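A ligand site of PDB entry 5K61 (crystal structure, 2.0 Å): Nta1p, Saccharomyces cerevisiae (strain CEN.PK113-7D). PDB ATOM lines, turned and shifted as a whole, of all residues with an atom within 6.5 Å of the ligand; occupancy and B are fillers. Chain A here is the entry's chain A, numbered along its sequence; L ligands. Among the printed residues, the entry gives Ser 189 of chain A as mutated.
CD2 of Tyr 142 touches N2 of the ligand (3.0 Å).
Met 190 touches the ligand.
Ser 193 touches the ligand (OG to N1, 3.9 Å).
Phe 197 touches the ligand (CZ to N1, 3.0 Å).
O of Ala 223 touches C4 of the ligand (3.1 Å).
Trp 224 touches the ligand.
Hydrophobic or aromatic side chains within 4 Å of the ligand: Tyr 71, Tyr 142, Met 190, Phe 197, Trp 224 and Leu 225.
Within 4 Å of the ligand: Tyr 71, Lys 138, Tyr 142, Ser 189, Met 190, Ser 193, Phe 197, Ala 223, Trp 224 and Leu 225.
N of Ala 223 lies within hydrogen-bond range of OE1 of Glu 65 (3.0 Å).
The side-chain carboxylate (OE1) of Glu 145 is in salt-bridge range of the side-chain amino group (NZ) of Lys 138, at 3.0 Å.
The side-chain carboxylate of Glu 65 lies within salt-bridge range of the side-chain amino group of Lys 138, 2.7 Å away.
The backbone NH of Lys 138 lies within hydrogen-bond range of the backbone carbonyl oxygen of Asn 121 (2.7 Å).
The side-chain carboxylate of Glu 65 is in hydrogen-bond range of the side-chain hydroxyl of Ser 189, at 2.6 Å.
O of Leu 225 lies within hydrogen-bond range of ND2 of Asn 299 (3.0 Å).
OG of Ser 189 is in hydrogen-bond range of NZ of Lys 138, at 3.0 Å.
OE1 of Glu 145 is in hydrogen-bond range of N of Tyr 142, at 2.9 Å.
NZ of Lys 138 lies within hydrogen-bond range of O2 of the ligand, 2.7 Å away.
OH of Tyr 71 sits at hydrogen-bond distance from N2 of the ligand (2.6 Å).
O1 of the ligand is in hydrogen-bond range of N of Leu 225.
The side-chain hydroxyl (OG) of Ser 189 sits at hydrogen-bond distance from an oxygen (O2) of the ligand, at 2.7 Å.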
ATOM      1  N   GLU A  65       3.846  -8.487 -21.477  1.00  0.00           N
ATOM      2  CA  GLU A  65       4.703  -9.586 -21.882  1.00  0.00           C
ATOM      3  C   GLU A  65       5.637  -9.915 -20.738  1.00  0.00           C
ATOM      4  O   GLU A  65       6.171  -9.015 -20.113  1.00  0.00           O
ATOM      5  CB  GLU A  65       5.479  -9.201 -23.149  1.00  0.00           C
ATOM      6  CG  GLU A  65       6.539 -10.183 -23.632  1.00  0.00           C
ATOM      7  CD  GLU A  65       7.078  -9.785 -25.004  1.00  0.00           C
ATOM      8  OE1 GLU A  65       6.708  -8.691 -25.496  1.00  0.00           O
ATOM      9  OE2 GLU A  65       7.853 -10.553 -25.607  1.00  0.00           O
ATOM     10  N   TYR A  71      12.435  -9.624 -18.571  1.00  0.00           N
ATOM     11  CA  TYR A  71      12.400  -9.890 -19.999  1.00  0.00           C
ATOM     12  C   TYR A  71      13.737 -10.296 -20.609  1.00  0.00           C
ATOM     13  O   TYR A  71      13.797 -11.202 -21.442  1.00  0.00           O
ATOM     14  CB  TYR A  71      11.859  -8.662 -20.769  1.00  0.00           C
ATOM     15  CG  TYR A  71      11.829  -8.923 -22.268  1.00  0.00           C
ATOM     16  CD1 TYR A  71      10.841  -9.724 -22.814  1.00  0.00           C
ATOM     17  CD2 TYR A  71      12.823  -8.424 -23.111  1.00  0.00           C
ATOM     18  CE1 TYR A  71      10.809 -10.007 -24.165  1.00  0.00           C
ATOM     19  CE2 TYR A  71      12.795  -8.693 -24.479  1.00  0.00           C
ATOM     20  CZ  TYR A  71      11.785  -9.493 -24.990  1.00  0.00           C
ATOM     21  OH  TYR A  71      11.727  -9.796 -26.327  1.00  0.00           O
ATOM     22  N   ASN A 121       7.306 -17.869 -25.456  1.00  0.00           N
ATOM     23  CA  ASN A 121       6.899 -16.539 -25.025  1.00  0.00           C
ATOM     24  C   ASN A 121       5.420 -16.439 -25.334  1.00  0.00           C
ATOM     25  O   ASN A 121       5.053 -16.418 -26.461  1.00  0.00           O
ATOM     26  CB  ASN A 121       7.699 -15.441 -25.724  1.00  0.00           C
ATOM     27  CG  ASN A 121       7.380 -14.057 -25.180  1.00  0.00           C
ATOM     28  OD1 ASN A 121       6.339 -13.840 -24.566  1.00  0.00           O
ATOM     29  ND2 ASN A 121       8.286 -13.112 -25.415  1.00  0.00           N
ATOM     30  N   LYS A 138       3.990 -16.285 -28.905  1.00  0.00           N
ATOM     31  CA  LYS A 138       4.525 -15.211 -29.744  1.00  0.00           C
ATOM     32  C   LYS A 138       4.946 -15.773 -31.121  1.00  0.00           C
ATOM     33  O   LYS A 138       5.494 -16.893 -31.220  1.00  0.00           O
ATOM     34  CB  LYS A 138       5.694 -14.526 -29.033  1.00  0.00           C
ATOM     35  CG  LYS A 138       6.173 -13.193 -29.645  1.00  0.00           C
ATOM     36  CD  LYS A 138       7.346 -12.642 -28.792  1.00  0.00           C
ATOM     37  CE  LYS A 138       7.720 -11.223 -29.215  1.00  0.00           C
ATOM     38  NZ  LYS A 138       8.658 -10.591 -28.220  1.00  0.00           N
ATOM     39  N   PHE A 140       6.114 -13.542 -34.107  1.00  0.00           N
ATOM     40  CA  PHE A 140       7.324 -12.860 -34.572  1.00  0.00           C
ATOM     41  C   PHE A 140       8.224 -12.628 -33.367  1.00  0.00           C
ATOM     42  O   PHE A 140       7.852 -11.906 -32.435  1.00  0.00           O
ATOM     43  CB  PHE A 140       6.996 -11.520 -35.236  1.00  0.00           C
ATOM     44  CG  PHE A 140       6.292 -11.639 -36.573  1.00  0.00           C
ATOM     45  CD1 PHE A 140       6.031 -12.868 -37.140  1.00  0.00           C
ATOM     46  CD2 PHE A 140       5.911 -10.499 -37.261  1.00  0.00           C
ATOM     47  CE1 PHE A 140       5.386 -12.968 -38.354  1.00  0.00           C
ATOM     48  CE2 PHE A 140       5.282 -10.580 -38.498  1.00  0.00           C
ATOM     49  CZ  PHE A 140       5.008 -11.815 -39.039  1.00  0.00           C
ATOM     50  N   LEU A 141       9.418 -13.214 -33.379  1.00  0.00           N
ATOM     51  CA  LEU A 141      10.312 -13.116 -32.226  1.00  0.00           C
ATOM     52  C   LEU A 141      11.295 -11.947 -32.383  1.00  0.00           C
ATOM     53  O   LEU A 141      11.664 -11.557 -33.488  1.00  0.00           O
ATOM     54  CB  LEU A 141      11.081 -14.425 -32.020  1.00  0.00           C
ATOM     55  CG  LEU A 141      10.278 -15.730 -31.961  1.00  0.00           C
ATOM     56  CD1 LEU A 141      11.213 -16.899 -31.602  1.00  0.00           C
ATOM     57  CD2 LEU A 141       9.120 -15.633 -30.965  1.00  0.00           C
ATOM     58  N   TYR A 142      11.710 -11.418 -31.239  1.00  0.00           N
ATOM     59  CA  TYR A 142      12.681 -10.337 -31.164  1.00  0.00           C
ATOM     60  C   TYR A 142      14.058 -10.952 -30.876  1.00  0.00           C
ATOM     61  O   TYR A 142      14.142 -12.115 -30.486  1.00  0.00           O
ATOM     62  CB  TYR A 142      12.261  -9.328 -30.077  1.00  0.00           C
ATOM     63  CG  TYR A 142      13.179  -8.140 -29.898  1.00  0.00           C
ATOM     64  CD1 TYR A 142      13.345  -7.202 -30.912  1.00  0.00           C
ATOM     65  CD2 TYR A 142      13.879  -7.938 -28.708  1.00  0.00           C
ATOM     66  CE1 TYR A 142      14.181  -6.112 -30.753  1.00  0.00           C
ATOM     67  CE2 TYR A 142      14.725  -6.840 -28.532  1.00  0.00           C
ATOM     68  CZ  TYR A 142      14.876  -5.936 -29.572  1.00  0.00           C
ATOM     69  OH  TYR A 142      15.718  -4.866 -29.426  1.00  0.00           O
ATOM     70  N   ASP A 143      15.131 -10.180 -31.095  1.00  0.00           N
ATOM     71  CA  ASP A 143      16.501 -10.659 -30.881  1.00  0.00           C
ATOM     72  C   ASP A 143      16.701 -11.344 -29.527  1.00  0.00           C
ATOM     73  O   ASP A 143      17.327 -12.392 -29.443  1.00  0.00           O
ATOM     74  CB  ASP A 143      17.483  -9.483 -31.007  1.00  0.00           C
ATOM     75  N   THR A 144      16.160 -10.753 -28.467  1.00  0.00           N
ATOM     76  CA  THR A 144      16.304 -11.317 -27.130  1.00  0.00           C
ATOM     77  C   THR A 144      15.836 -12.772 -27.023  1.00  0.00           C
ATOM     78  O   THR A 144      16.456 -13.566 -26.323  1.00  0.00           O
ATOM     79  CB  THR A 144      15.535 -10.466 -26.105  1.00  0.00           C
ATOM     80  OG1 THR A 144      15.955  -9.103 -26.250  1.00  0.00           O
ATOM     81  CG2 THR A 144      15.831 -10.927 -24.686  1.00  0.00           C
ATOM     82  N   GLU A 145      14.739 -13.118 -27.684  1.00  0.00           N
ATOM     83  CA  GLU A 145      14.209 -14.488 -27.620  1.00  0.00           C
ATOM     84  C   GLU A 145      15.215 -15.501 -28.162  1.00  0.00           C
ATOM     85  O   GLU A 145      15.213 -16.673 -27.762  1.00  0.00           O
ATOM     86  CB  GLU A 145      12.909 -14.620 -28.408  1.00  0.00           C
ATOM     87  CG  GLU A 145      11.665 -14.395 -27.579  1.00  0.00           C
ATOM     88  CD  GLU A 145      11.302 -12.946 -27.501  1.00  0.00           C
ATOM     89  OE1 GLU A 145      11.070 -12.344 -28.578  1.00  0.00           O
ATOM     90  OE2 GLU A 145      11.261 -12.400 -26.381  1.00  0.00           O
ATOM     91  N   ILE A 188       1.689 -10.453 -29.240  1.00  0.00           N
ATOM     92  CA  ILE A 188       2.748 -10.114 -28.275  1.00  0.00           C
ATOM     93  C   ILE A 188       3.833  -9.258 -28.965  1.00  0.00           C
ATOM     94  O   ILE A 188       4.443  -9.700 -29.940  1.00  0.00           O
ATOM     95  CB  ILE A 188       3.357 -11.395 -27.652  1.00  0.00           C
ATOM     96  CG1 ILE A 188       2.269 -12.208 -26.929  1.00  0.00           C
ATOM     97  CG2 ILE A 188       4.496 -11.070 -26.696  1.00  0.00           C
ATOM     98  CD1 ILE A 188       2.742 -13.566 -26.379  1.00  0.00           C
ATOM     99  N   SER A 189       4.020  -8.046 -28.440  1.00  0.00           N
ATOM    100  CA  SER A 189       4.940  -7.009 -28.943  1.00  0.00           C
ATOM    101  C   SER A 189       5.424  -7.116 -30.401  1.00  0.00           C
ATOM    102  O   SER A 189       4.801  -6.572 -31.295  1.00  0.00           O
ATOM    103  CB  SER A 189       6.171  -6.930 -28.031  1.00  0.00           C
ATOM    104  OG  SER A 189       6.934  -8.131 -28.054  1.00  0.00           O
ATOM    105  N   MET A 190       6.546  -7.799 -30.618  1.00  0.00           N
ATOM    106  CA  MET A 190       7.142  -7.921 -31.949  1.00  0.00           C
ATOM    107  C   MET A 190       6.161  -8.441 -33.014  1.00  0.00           C
ATOM    108  O   MET A 190       6.395  -8.222 -34.211  1.00  0.00           O
ATOM    109  CB  MET A 190       8.365  -8.832 -31.900  1.00  0.00           C
ATOM    110  CG  MET A 190       9.110  -8.978 -33.228  1.00  0.00           C
ATOM    111  SD  MET A 190      10.218  -7.599 -33.543  1.00  0.00           S
ATOM    112  CE  MET A 190      10.906  -7.978 -35.163  1.00  0.00           C
ATOM    113  N   ASP A 191       5.097  -9.130 -32.601  1.00  0.00           N
ATOM    114  CA  ASP A 191       4.059  -9.554 -33.543  1.00  0.00           C
ATOM    115  C   ASP A 191       3.599  -8.394 -34.397  1.00  0.00           C
ATOM    116  O   ASP A 191       3.251  -8.576 -35.563  1.00  0.00           O
ATOM    117  CB  ASP A 191       2.835 -10.145 -32.818  1.00  0.00           C
ATOM    118  CG  ASP A 191       3.092 -11.557 -32.293  1.00  0.00           C
ATOM    119  OD1 ASP A 191       4.094 -12.185 -32.714  1.00  0.00           O
ATOM    120  OD2 ASP A 191       2.297 -12.042 -31.461  1.00  0.00           O
ATOM    121  N   SER A 193       5.400  -5.874 -35.529  1.00  0.00           N
ATOM    122  CA  SER A 193       6.486  -5.382 -36.385  1.00  0.00           C
ATOM    123  C   SER A 193       6.545  -6.128 -37.705  1.00  0.00           C
ATOM    124  O   SER A 193       5.994  -7.220 -37.824  1.00  0.00           O
ATOM    125  CB  SER A 193       7.848  -5.551 -35.688  1.00  0.00           C
ATOM    126  OG  SER A 193       7.855  -4.977 -34.393  1.00  0.00           O
ATOM    127  N   PHE A 197      11.983  -7.546 -38.656  1.00  0.00           N
ATOM    128  CA  PHE A 197      12.393  -6.189 -39.025  1.00  0.00           C
ATOM    129  C   PHE A 197      12.976  -6.156 -40.440  1.00  0.00           C
ATOM    130  O   PHE A 197      13.621  -5.176 -40.813  1.00  0.00           O
ATOM    131  CB  PHE A 197      13.446  -5.642 -38.048  1.00  0.00           C
ATOM    132  CG  PHE A 197      12.922  -5.324 -36.691  1.00  0.00           C
ATOM    133  CD1 PHE A 197      11.776  -4.574 -36.532  1.00  0.00           C
ATOM    134  CD2 PHE A 197      13.556  -5.811 -35.566  1.00  0.00           C
ATOM    135  CE1 PHE A 197      11.295  -4.273 -35.272  1.00  0.00           C
ATOM    136  CE2 PHE A 197      13.062  -5.517 -34.301  1.00  0.00           C
ATOM    137  CZ  PHE A 197      11.932  -4.748 -34.165  1.00  0.00           C
ATOM    138  N   ALA A 223       6.583  -5.982 -24.285  1.00  0.00           N
ATOM    139  CA  ALA A 223       7.784  -5.449 -23.641  1.00  0.00           C
ATOM    140  C   ALA A 223       8.487  -4.651 -24.729  1.00  0.00           C
ATOM    141  O   ALA A 223       9.463  -5.109 -25.321  1.00  0.00           O
ATOM    142  CB  ALA A 223       8.661  -6.552 -23.087  1.00  0.00           C
ATOM    143  N   TRP A 224       7.951  -3.471 -25.018  1.00  0.00           N
ATOM    144  CA  TRP A 224       8.306  -2.700 -26.204  1.00  0.00           C
ATOM    145  C   TRP A 224       9.227  -1.537 -25.817  1.00  0.00           C
ATOM    146  O   TRP A 224       8.970  -0.838 -24.835  1.00  0.00           O
ATOM    147  CB  TRP A 224       7.031  -2.178 -26.883  1.00  0.00           C
ATOM    148  CG  TRP A 224       7.276  -1.512 -28.199  1.00  0.00           C
ATOM    149  CD1 TRP A 224       7.721  -0.234 -28.402  1.00  0.00           C
ATOM    150  CD2 TRP A 224       7.048  -2.069 -29.500  1.00  0.00           C
ATOM    151  NE1 TRP A 224       7.799   0.033 -29.751  1.00  0.00           N
ATOM    152  CE2 TRP A 224       7.397  -1.078 -30.441  1.00  0.00           C
ATOM    153  CE3 TRP A 224       6.583  -3.313 -29.954  1.00  0.00           C
ATOM    154  CZ2 TRP A 224       7.299  -1.292 -31.825  1.00  0.00           C
ATOM    155  CZ3 TRP A 224       6.486  -3.527 -31.337  1.00  0.00           C
ATOM    156  CH2 TRP A 224       6.838  -2.512 -32.257  1.00  0.00           C
ATOM    157  N   LEU A 225      10.295  -1.339 -26.579  1.00  0.00           N
ATOM    158  CA  LEU A 225      11.345  -0.390 -26.221  1.00  0.00           C
ATOM    159  C   LEU A 225      11.069   1.075 -26.557  1.00  0.00           C
ATOM    160  O   LEU A 225      10.540   1.400 -27.612  1.00  0.00           O
ATOM    161  CB  LEU A 225      12.659  -0.779 -26.896  1.00  0.00           C
ATOM    162  CG  LEU A 225      13.543  -1.815 -26.197  1.00  0.00           C
ATOM    163  CD1 LEU A 225      12.741  -3.066 -25.916  1.00  0.00           C
ATOM    164  CD2 LEU A 225      14.758  -2.135 -27.063  1.00  0.00           C
ATOM    165  N   ASN A 226      11.458   1.950 -25.623  1.00  0.00           N
ATOM    166  CA  ASN A 226      11.652   3.367 -25.919  1.00  0.00           C
ATOM    167  C   ASN A 226      12.964   3.500 -26.731  1.00  0.00           C
ATOM    168  O   ASN A 226      13.914   2.748 -26.499  1.00  0.00           O
ATOM    169  CB  ASN A 226      11.696   4.163 -24.611  1.00  0.00           C
ATOM    170  CG  ASN A 226      12.182   5.584 -24.792  1.00  0.00           C
ATOM    171  OD1 ASN A 226      13.386   5.829 -24.847  1.00  0.00           O
ATOM    172  ND2 ASN A 226      11.246   6.531 -24.880  1.00  0.00           N
ATOM    173  N   ASN A 299       6.165   6.233 -29.533  1.00  0.00           N
ATOM    174  CA  ASN A 299       5.695   4.862 -29.632  1.00  0.00           C
ATOM    175  C   ASN A 299       4.184   4.755 -29.802  1.00  0.00           C
ATOM    176  O   ASN A 299       3.715   3.891 -30.543  1.00  0.00           O
ATOM    177  CB  ASN A 299       6.141   4.052 -28.432  1.00  0.00           C
ATOM    178  CG  ASN A 299       7.494   3.437 -28.656  1.00  0.00           C
ATOM    179  OD1 ASN A 299       7.793   2.950 -29.745  1.00  0.00           O
ATOM    180  ND2 ASN A 299       8.347   3.497 -27.651  1.00  0.00           N
ATOM    181  N   PHE A 403      12.174   0.237 -21.404  1.00  0.00           N
ATOM    182  CA  PHE A 403      10.841  -0.079 -21.929  1.00  0.00           C
ATOM    183  C   PHE A 403       9.955   1.162 -21.930  1.00  0.00           C
ATOM    184  O   PHE A 403      10.091   2.035 -21.069  1.00  0.00           O
ATOM    185  CB  PHE A 403      10.227  -1.233 -21.120  1.00  0.00           C
ATOM    186  CG  PHE A 403      11.019  -2.507 -21.220  1.00  0.00           C
ATOM    187  CD1 PHE A 403      10.935  -3.302 -22.355  1.00  0.00           C
ATOM    188  CD2 PHE A 403      11.888  -2.886 -20.216  1.00  0.00           C
ATOM    189  CE1 PHE A 403      11.689  -4.472 -22.475  1.00  0.00           C
ATOM    190  CE2 PHE A 403      12.623  -4.048 -20.327  1.00  0.00           C
ATOM    191  CZ  PHE A 403      12.529  -4.840 -21.463  1.00  0.00           C
HETATM  192  N1  LIG L   1      10.459  -3.987 -31.628  1.00  0.00           N
HETATM  193  C1  LIG L   1       9.960  -4.068 -30.260  1.00  0.00           C
HETATM  194  C2  LIG L   1      10.836  -3.303 -29.287  1.00  0.00           C
HETATM  195  O1  LIG L   1      10.562  -2.146 -28.999  1.00  0.00           O
HETATM  196  C3  LIG L   1       9.863  -5.523 -29.802  1.00  0.00           C
HETATM  197  C4  LIG L   1      10.170  -5.687 -28.329  1.00  0.00           C
HETATM  198  C5  LIG L   1      10.364  -7.141 -27.948  1.00  0.00           C
HETATM  199  O2  LIG L   1       9.618  -8.027 -28.372  1.00  0.00           O
HETATM  200  N2  LIG L   1      11.383  -7.400 -27.145  1.00  0.00           N
